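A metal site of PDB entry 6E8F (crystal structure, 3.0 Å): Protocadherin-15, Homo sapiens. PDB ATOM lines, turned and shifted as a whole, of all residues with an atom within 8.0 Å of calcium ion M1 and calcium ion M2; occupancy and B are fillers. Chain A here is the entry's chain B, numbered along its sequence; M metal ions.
Within 4 Å of calcium ion M2: Asn 128, Gln 130, Asp 169, Asp 171 and Asp 231.
Five residues have an atom within 4 Å of calcium ion M1: Asp 126, Glu 127, Asn 129, Gln 130 and Asp 171. The nearest printed residue that does not touch calcium ion M1 is Glu 27 (4.6 Å).
Calcium ion M2 is bound by the side-chain carboxylate (OD2) of Asp 169 (2.2 Å). OD2 of Asp 171 is bound to calcium ion M2, 2.3 Å away. OD2 of Asp 231 is bound to calcium ion M2, at 2.4 Å. The side-chain carboxylate (OD1) of Asp 169 is bound to calcium ion M2, 2.4 Å away. Calcium ion M2 is bound by the backbone carbonyl oxygen (O) of Gln 130 (2.5 Å). Calcium ion M2 is bound by OD1 of Asn 128, 2.5 Å away. Calcium ion M2 has six donor atoms within binding distance.
O of Glu 127 is bound to calcium ion M1, 2.4 Å away. Calcium ion M1 is bound by the side-chain carboxylate (OD1) of Asp 126 (2.4 Å). OD1 of Asp 171 is bound to calcium ion M1 (2.6 Å). OD1 of Asn 129 is bound to calcium ion M1.
The side-chain carboxylate of Asp 231 is in hydrogen-bond range of the backbone NH of Gln 234 (2.6 Å). OD1 of Asp 231 lies within hydrogen-bond range of N of Val 233 (2.7 Å). N of Gln 130 lies close to NE2 of Gln 234 (3.0 Å). O of Asn 128 lies close to OE1 of Gln 234 (3.3 Å). The backbone carbonyl oxygen (O) of Asn 129 sits close to the side-chain amide nitrogen (NE2) of Gln 234 (3.2 Å).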
ATOM      1  N   GLU A  27     -14.051  -9.219 -30.458  1.00  0.00           N
ATOM      2  CA  GLU A  27     -14.889  -8.554 -29.473  1.00  0.00           C
ATOM      3  C   GLU A  27     -14.235  -8.731 -28.099  1.00  0.00           C
ATOM      4  O   GLU A  27     -13.467  -9.657 -27.897  1.00  0.00           O
ATOM      5  CB  GLU A  27     -16.316  -9.114 -29.466  1.00  0.00           C
ATOM      6  CG  GLU A  27     -16.429 -10.535 -28.929  1.00  0.00           C
ATOM      7  CD  GLU A  27     -17.812 -10.945 -28.459  1.00  0.00           C
ATOM      8  OE1 GLU A  27     -18.126 -12.174 -28.511  1.00  0.00           O
ATOM      9  OE2 GLU A  27     -18.585 -10.058 -28.022  1.00  0.00           O
ATOM     10  N   LEU A  28     -14.507  -7.766 -27.210  1.00  0.00           N
ATOM     11  CA  LEU A  28     -14.308  -7.882 -25.774  1.00  0.00           C
ATOM     12  C   LEU A  28     -12.855  -7.622 -25.363  1.00  0.00           C
ATOM     13  O   LEU A  28     -12.627  -7.276 -24.217  1.00  0.00           O
ATOM     14  CB  LEU A  28     -14.784  -9.251 -25.282  1.00  0.00           C
ATOM     15  CG  LEU A  28     -16.286  -9.482 -25.396  1.00  0.00           C
ATOM     16  CD1 LEU A  28     -16.700 -10.734 -24.632  1.00  0.00           C
ATOM     17  CD2 LEU A  28     -17.073  -8.277 -24.906  1.00  0.00           C
ATOM     18  N   ARG A  94     -19.864  -7.816 -29.369  1.00  0.00           N
ATOM     19  CA  ARG A  94     -20.401  -8.253 -30.678  1.00  0.00           C
ATOM     20  C   ARG A  94     -21.927  -8.289 -30.686  1.00  0.00           C
ATOM     21  O   ARG A  94     -22.556  -8.030 -31.737  1.00  0.00           O
ATOM     22  CB  ARG A  94     -19.896  -9.646 -31.054  1.00  0.00           C
ATOM     23  CG  ARG A  94     -20.187 -10.029 -32.499  1.00  0.00           C
ATOM     24  CD  ARG A  94     -19.335 -11.189 -32.974  1.00  0.00           C
ATOM     25  NE  ARG A  94     -19.516 -11.494 -34.385  1.00  0.00           N
ATOM     26  CZ  ARG A  94     -20.637 -11.974 -34.898  1.00  0.00           C
ATOM     27  NH1 ARG A  94     -21.567 -12.456 -34.093  1.00  0.00           N
ATOM     28  NH2 ARG A  94     -20.836 -11.932 -36.194  1.00  0.00           N
ATOM     29  N   LEU A 125     -15.224  -9.896 -34.643  1.00  0.00           N
ATOM     30  CA  LEU A 125     -15.106 -11.341 -34.676  1.00  0.00           C
ATOM     31  C   LEU A 125     -15.500 -11.936 -33.309  1.00  0.00           C
ATOM     32  O   LEU A 125     -15.201 -11.349 -32.261  1.00  0.00           O
ATOM     33  CB  LEU A 125     -13.649 -11.702 -35.004  1.00  0.00           C
ATOM     34  CG  LEU A 125     -13.133 -11.178 -36.341  1.00  0.00           C
ATOM     35  CD1 LEU A 125     -11.733 -11.696 -36.625  1.00  0.00           C
ATOM     36  CD2 LEU A 125     -14.088 -11.526 -37.468  1.00  0.00           C
ATOM     37  N   ASP A 126     -16.157 -13.093 -33.349  1.00  0.00           N
ATOM     38  CA  ASP A 126     -16.323 -13.924 -32.175  1.00  0.00           C
ATOM     39  C   ASP A 126     -14.987 -14.623 -31.940  1.00  0.00           C
ATOM     40  O   ASP A 126     -14.527 -15.404 -32.766  1.00  0.00           O
ATOM     41  CB  ASP A 126     -17.484 -14.920 -32.321  1.00  0.00           C
ATOM     42  CG  ASP A 126     -17.945 -15.548 -31.020  1.00  0.00           C
ATOM     43  OD1 ASP A 126     -17.079 -15.863 -30.172  1.00  0.00           O
ATOM     44  OD2 ASP A 126     -19.167 -15.715 -30.855  1.00  0.00           O
ATOM     45  N   GLU A 127     -14.323 -14.280 -30.836  1.00  0.00           N
ATOM     46  CA  GLU A 127     -13.067 -14.917 -30.521  1.00  0.00           C
ATOM     47  C   GLU A 127     -13.383 -16.397 -30.238  1.00  0.00           C
ATOM     48  O   GLU A 127     -14.378 -16.681 -29.548  1.00  0.00           O
ATOM     49  CB  GLU A 127     -12.417 -14.155 -29.350  1.00  0.00           C
ATOM     50  CG  GLU A 127     -10.903 -14.139 -29.376  1.00  0.00           C
ATOM     51  CD  GLU A 127     -10.265 -13.652 -28.086  1.00  0.00           C
ATOM     52  OE1 GLU A 127     -11.011 -13.249 -27.157  1.00  0.00           O
ATOM     53  OE2 GLU A 127      -9.022 -13.671 -28.011  1.00  0.00           O
ATOM     54  N   ASN A 128     -12.598 -17.309 -30.837  1.00  0.00           N
ATOM     55  CA  ASN A 128     -12.657 -18.748 -30.525  1.00  0.00           C
ATOM     56  C   ASN A 128     -11.891 -19.004 -29.225  1.00  0.00           C
ATOM     57  O   ASN A 128     -10.815 -19.587 -29.226  1.00  0.00           O
ATOM     58  CB  ASN A 128     -12.123 -19.635 -31.647  1.00  0.00           C
ATOM     59  CG  ASN A 128     -12.010 -21.102 -31.264  1.00  0.00           C
ATOM     60  OD1 ASN A 128     -12.527 -21.537 -30.228  1.00  0.00           O
ATOM     61  ND2 ASN A 128     -11.325 -21.884 -32.089  1.00  0.00           N
ATOM     62  N   ASN A 129     -12.472 -18.532 -28.120  1.00  0.00           N
ATOM     63  CA  ASN A 129     -11.899 -18.694 -26.811  1.00  0.00           C
ATOM     64  C   ASN A 129     -12.894 -19.445 -25.928  1.00  0.00           C
ATOM     65  O   ASN A 129     -12.778 -19.400 -24.714  1.00  0.00           O
ATOM     66  CB  ASN A 129     -11.557 -17.338 -26.199  1.00  0.00           C
ATOM     67  CG  ASN A 129     -12.782 -16.537 -25.819  1.00  0.00           C
ATOM     68  OD1 ASN A 129     -13.772 -16.508 -26.539  1.00  0.00           O
ATOM     69  ND2 ASN A 129     -12.712 -15.883 -24.667  1.00  0.00           N
ATOM     70  N   GLN A 130     -13.856 -20.149 -26.544  1.00  0.00           N
ATOM     71  CA  GLN A 130     -14.770 -21.029 -25.825  1.00  0.00           C
ATOM     72  C   GLN A 130     -14.591 -22.486 -26.284  1.00  0.00           C
ATOM     73  O   GLN A 130     -14.402 -22.827 -27.476  1.00  0.00           O
ATOM     74  CB  GLN A 130     -16.224 -20.583 -25.981  1.00  0.00           C
ATOM     75  CG  GLN A 130     -16.529 -19.231 -25.346  1.00  0.00           C
ATOM     76  CD  GLN A 130     -17.883 -19.203 -24.668  1.00  0.00           C
ATOM     77  OE1 GLN A 130     -18.139 -19.935 -23.709  1.00  0.00           O
ATOM     78  NE2 GLN A 130     -18.759 -18.338 -25.146  1.00  0.00           N
ATOM     79  N   SER A 131     -14.693 -23.358 -25.273  1.00  0.00           N
ATOM     80  CA  SER A 131     -14.329 -24.751 -25.330  1.00  0.00           C
ATOM     81  C   SER A 131     -15.559 -25.586 -25.664  1.00  0.00           C
ATOM     82  O   SER A 131     -16.582 -25.470 -24.993  1.00  0.00           O
ATOM     83  CB  SER A 131     -13.752 -25.144 -23.999  1.00  0.00           C
ATOM     84  OG  SER A 131     -12.846 -26.198 -24.154  1.00  0.00           O
ATOM     85  N   PRO A 132     -15.514 -26.466 -26.683  1.00  0.00           N
ATOM     86  CA  PRO A 132     -16.715 -27.206 -27.100  1.00  0.00           C
ATOM     87  C   PRO A 132     -17.186 -28.112 -25.954  1.00  0.00           C
ATOM     88  O   PRO A 132     -16.403 -28.425 -25.051  1.00  0.00           O
ATOM     89  CB  PRO A 132     -16.271 -27.997 -28.325  1.00  0.00           C
ATOM     90  CG  PRO A 132     -14.764 -28.148 -28.136  1.00  0.00           C
ATOM     91  CD  PRO A 132     -14.321 -26.887 -27.428  1.00  0.00           C
ATOM     92  N   TYR A 133     -18.466 -28.509 -25.984  1.00  0.00           N
ATOM     93  CA  TYR A 133     -19.058 -29.282 -24.906  1.00  0.00           C
ATOM     94  C   TYR A 133     -20.022 -30.309 -25.485  1.00  0.00           C
ATOM     95  O   TYR A 133     -20.572 -30.112 -26.555  1.00  0.00           O
ATOM     96  CB  TYR A 133     -19.737 -28.344 -23.900  1.00  0.00           C
ATOM     97  CG  TYR A 133     -20.896 -27.560 -24.465  1.00  0.00           C
ATOM     98  CD1 TYR A 133     -20.706 -26.322 -25.067  1.00  0.00           C
ATOM     99  CD2 TYR A 133     -22.192 -28.061 -24.421  1.00  0.00           C
ATOM    100  CE1 TYR A 133     -21.763 -25.611 -25.596  1.00  0.00           C
ATOM    101  CE2 TYR A 133     -23.259 -27.361 -24.952  1.00  0.00           C
ATOM    102  CZ  TYR A 133     -23.051 -26.121 -25.541  1.00  0.00           C
ATOM    103  OH  TYR A 133     -24.103 -25.430 -26.090  1.00  0.00           O
ATOM    104  N   LEU A 168     -21.333 -29.054 -29.192  1.00  0.00           N
ATOM    105  CA  LEU A 168     -21.602 -27.670 -29.577  1.00  0.00           C
ATOM    106  C   LEU A 168     -20.467 -26.766 -29.094  1.00  0.00           C
ATOM    107  O   LEU A 168     -19.578 -27.216 -28.370  1.00  0.00           O
ATOM    108  CB  LEU A 168     -22.937 -27.247 -28.949  1.00  0.00           C
ATOM    109  CG  LEU A 168     -24.140 -28.119 -29.301  1.00  0.00           C
ATOM    110  CD1 LEU A 168     -25.314 -27.710 -28.430  1.00  0.00           C
ATOM    111  CD2 LEU A 168     -24.491 -28.025 -30.786  1.00  0.00           C
ATOM    112  N   ASP A 169     -20.501 -25.503 -29.491  1.00  0.00           N
ATOM    113  CA  ASP A 169     -19.425 -24.579 -29.191  1.00  0.00           C
ATOM    114  C   ASP A 169     -19.995 -23.161 -29.182  1.00  0.00           C
ATOM    115  O   ASP A 169     -20.390 -22.671 -30.220  1.00  0.00           O
ATOM    116  CB  ASP A 169     -18.281 -24.735 -30.219  1.00  0.00           C
ATOM    117  CG  ASP A 169     -17.015 -23.957 -29.890  1.00  0.00           C
ATOM    118  OD1 ASP A 169     -17.104 -22.757 -29.639  1.00  0.00           O
ATOM    119  OD2 ASP A 169     -15.937 -24.570 -29.892  1.00  0.00           O
ATOM    120  N   LYS A 170     -20.021 -22.535 -27.998  1.00  0.00           N
ATOM    121  CA  LYS A 170     -20.607 -21.163 -27.831  1.00  0.00           C
ATOM    122  C   LYS A 170     -20.144 -20.229 -28.946  1.00  0.00           C
ATOM    123  O   LYS A 170     -20.968 -19.556 -29.566  1.00  0.00           O
ATOM    124  CB  LYS A 170     -20.235 -20.580 -26.465  1.00  0.00           C
ATOM    125  CG  LYS A 170     -20.812 -21.316 -25.260  1.00  0.00           C
ATOM    126  CD  LYS A 170     -22.245 -20.942 -24.958  1.00  0.00           C
ATOM    127  CE  LYS A 170     -23.149 -22.128 -24.709  1.00  0.00           C
ATOM    128  NZ  LYS A 170     -23.627 -22.743 -25.984  1.00  0.00           N
ATOM    129  N   ASP A 171     -18.829 -20.212 -29.222  1.00  0.00           N
ATOM    130  CA  ASP A 171     -18.196 -19.357 -30.228  1.00  0.00           C
ATOM    131  C   ASP A 171     -18.945 -19.360 -31.567  1.00  0.00           C
ATOM    132  O   ASP A 171     -18.896 -18.381 -32.288  1.00  0.00           O
ATOM    133  CB  ASP A 171     -16.756 -19.792 -30.491  1.00  0.00           C
ATOM    134  CG  ASP A 171     -15.858 -19.733 -29.265  1.00  0.00           C
ATOM    135  OD1 ASP A 171     -16.040 -18.819 -28.454  1.00  0.00           O
ATOM    136  OD2 ASP A 171     -14.995 -20.619 -29.146  1.00  0.00           O
ATOM    137  N   ILE A 172     -19.588 -20.477 -31.918  1.00  0.00           N
ATOM    138  CA  ILE A 172     -20.239 -20.654 -33.217  1.00  0.00           C
ATOM    139  C   ILE A 172     -21.750 -20.391 -33.106  1.00  0.00           C
ATOM    140  O   ILE A 172     -22.344 -19.841 -34.026  1.00  0.00           O
ATOM    141  CB  ILE A 172     -19.932 -22.047 -33.792  1.00  0.00           C
ATOM    142  CG1 ILE A 172     -18.482 -22.153 -34.293  1.00  0.00           C
ATOM    143  CG2 ILE A 172     -20.944 -22.440 -34.871  1.00  0.00           C
ATOM    144  CD1 ILE A 172     -18.280 -21.782 -35.746  1.00  0.00           C
ATOM    145  N   PRO A 185     -20.519 -26.650 -35.938  1.00  0.00           N
ATOM    146  CA  PRO A 185     -19.279 -26.007 -35.528  1.00  0.00           C
ATOM    147  C   PRO A 185     -17.981 -26.678 -36.021  1.00  0.00           C
ATOM    148  O   PRO A 185     -16.900 -26.290 -35.581  1.00  0.00           O
ATOM    149  CB  PRO A 185     -19.369 -26.060 -33.990  1.00  0.00           C
ATOM    150  CG  PRO A 185     -20.195 -27.302 -33.698  1.00  0.00           C
ATOM    151  CD  PRO A 185     -21.122 -27.484 -34.885  1.00  0.00           C
ATOM    152  N   LEU A 187     -16.240 -29.330 -35.504  1.00  0.00           N
ATOM    153  CA  LEU A 187     -15.329 -29.815 -34.503  1.00  0.00           C
ATOM    154  C   LEU A 187     -14.713 -31.136 -34.957  1.00  0.00           C
ATOM    155  O   LEU A 187     -15.182 -31.740 -35.905  1.00  0.00           O
ATOM    156  CB  LEU A 187     -16.103 -30.058 -33.211  1.00  0.00           C
ATOM    157  CG  LEU A 187     -16.778 -28.837 -32.619  1.00  0.00           C
ATOM    158  CD1 LEU A 187     -17.810 -29.293 -31.608  1.00  0.00           C
ATOM    159  CD2 LEU A 187     -15.730 -27.914 -32.008  1.00  0.00           C
ATOM    160  N   PHE A 230     -12.653 -31.139 -30.049  1.00  0.00           N
ATOM    161  CA  PHE A 230     -11.561 -30.217 -30.326  1.00  0.00           C
ATOM    162  C   PHE A 230     -12.031 -29.222 -31.386  1.00  0.00           C
ATOM    163  O   PHE A 230     -12.665 -29.627 -32.355  1.00  0.00           O
ATOM    164  CB  PHE A 230     -10.331 -30.953 -30.865  1.00  0.00           C
ATOM    165  CG  PHE A 230      -9.174 -30.044 -31.212  1.00  0.00           C
ATOM    166  CD1 PHE A 230      -8.570 -29.269 -30.232  1.00  0.00           C
ATOM    167  CD2 PHE A 230      -8.704 -29.947 -32.505  1.00  0.00           C
ATOM    168  CE1 PHE A 230      -7.514 -28.439 -30.550  1.00  0.00           C
ATOM    169  CE2 PHE A 230      -7.648 -29.107 -32.823  1.00  0.00           C
ATOM    170  CZ  PHE A 230      -7.042 -28.362 -31.844  1.00  0.00           C
ATOM    171  N   ASP A 231     -11.677 -27.943 -31.192  1.00  0.00           N
ATOM    172  CA  ASP A 231     -12.280 -26.866 -31.957  1.00  0.00           C
ATOM    173  C   ASP A 231     -11.199 -26.082 -32.711  1.00  0.00           C
ATOM    174  O   ASP A 231     -11.448 -24.994 -33.197  1.00  0.00           O
ATOM    175  CB  ASP A 231     -13.104 -25.937 -31.050  1.00  0.00           C
ATOM    176  CG  ASP A 231     -12.300 -24.962 -30.187  1.00  0.00           C
ATOM    177  OD1 ASP A 231     -11.051 -24.914 -30.341  1.00  0.00           O
ATOM    178  OD2 ASP A 231     -12.943 -24.236 -29.397  1.00  0.00           O
ATOM    179  N   GLY A 232      -9.995 -26.662 -32.800  1.00  0.00           N
ATOM    180  CA  GLY A 232      -8.867 -26.008 -33.428  1.00  0.00           C
ATOM    181  C   GLY A 232      -7.976 -25.321 -32.420  1.00  0.00           C
ATOM    182  O   GLY A 232      -6.776 -25.214 -32.662  1.00  0.00           O
ATOM    183  N   VAL A 233      -8.540 -24.900 -31.273  1.00  0.00           N
ATOM    184  CA  VAL A 233      -7.795 -24.207 -30.199  1.00  0.00           C
ATOM    185  C   VAL A 233      -8.012 -24.877 -28.824  1.00  0.00           C
ATOM    186  O   VAL A 233      -7.090 -24.954 -28.047  1.00  0.00           O
ATOM    187  CB  VAL A 233      -8.171 -22.713 -30.171  1.00  0.00           C
ATOM    188  CG1 VAL A 233      -7.641 -21.992 -28.942  1.00  0.00           C
ATOM    189  CG2 VAL A 233      -7.734 -22.017 -31.434  1.00  0.00           C
ATOM    190  N   GLN A 234      -9.223 -25.309 -28.496  1.00  0.00           N
ATOM    191  CA  GLN A 234      -9.456 -25.879 -27.180  1.00  0.00           C
ATOM    192  C   GLN A 234     -10.051 -27.280 -27.291  1.00  0.00           C
ATOM    193  O   GLN A 234     -10.697 -27.616 -28.280  1.00  0.00           O
ATOM    194  CB  GLN A 234     -10.403 -24.998 -26.358  1.00  0.00           C
ATOM    195  CG  GLN A 234      -9.894 -23.575 -26.181  1.00  0.00           C
ATOM    196  CD  GLN A 234     -10.650 -22.618 -27.061  1.00  0.00           C
ATOM    197  OE1 GLN A 234     -10.726 -22.780 -28.273  1.00  0.00           O
ATOM    198  NE2 GLN A 234     -11.225 -21.621 -26.420  1.00  0.00           N
HETATM  199 CA    CA M   1     -16.159 -16.273 -27.945  1.00  0.00          CA
HETATM  200 CA    CA M   2     -14.697 -22.750 -29.908  1.00  0.00          CA
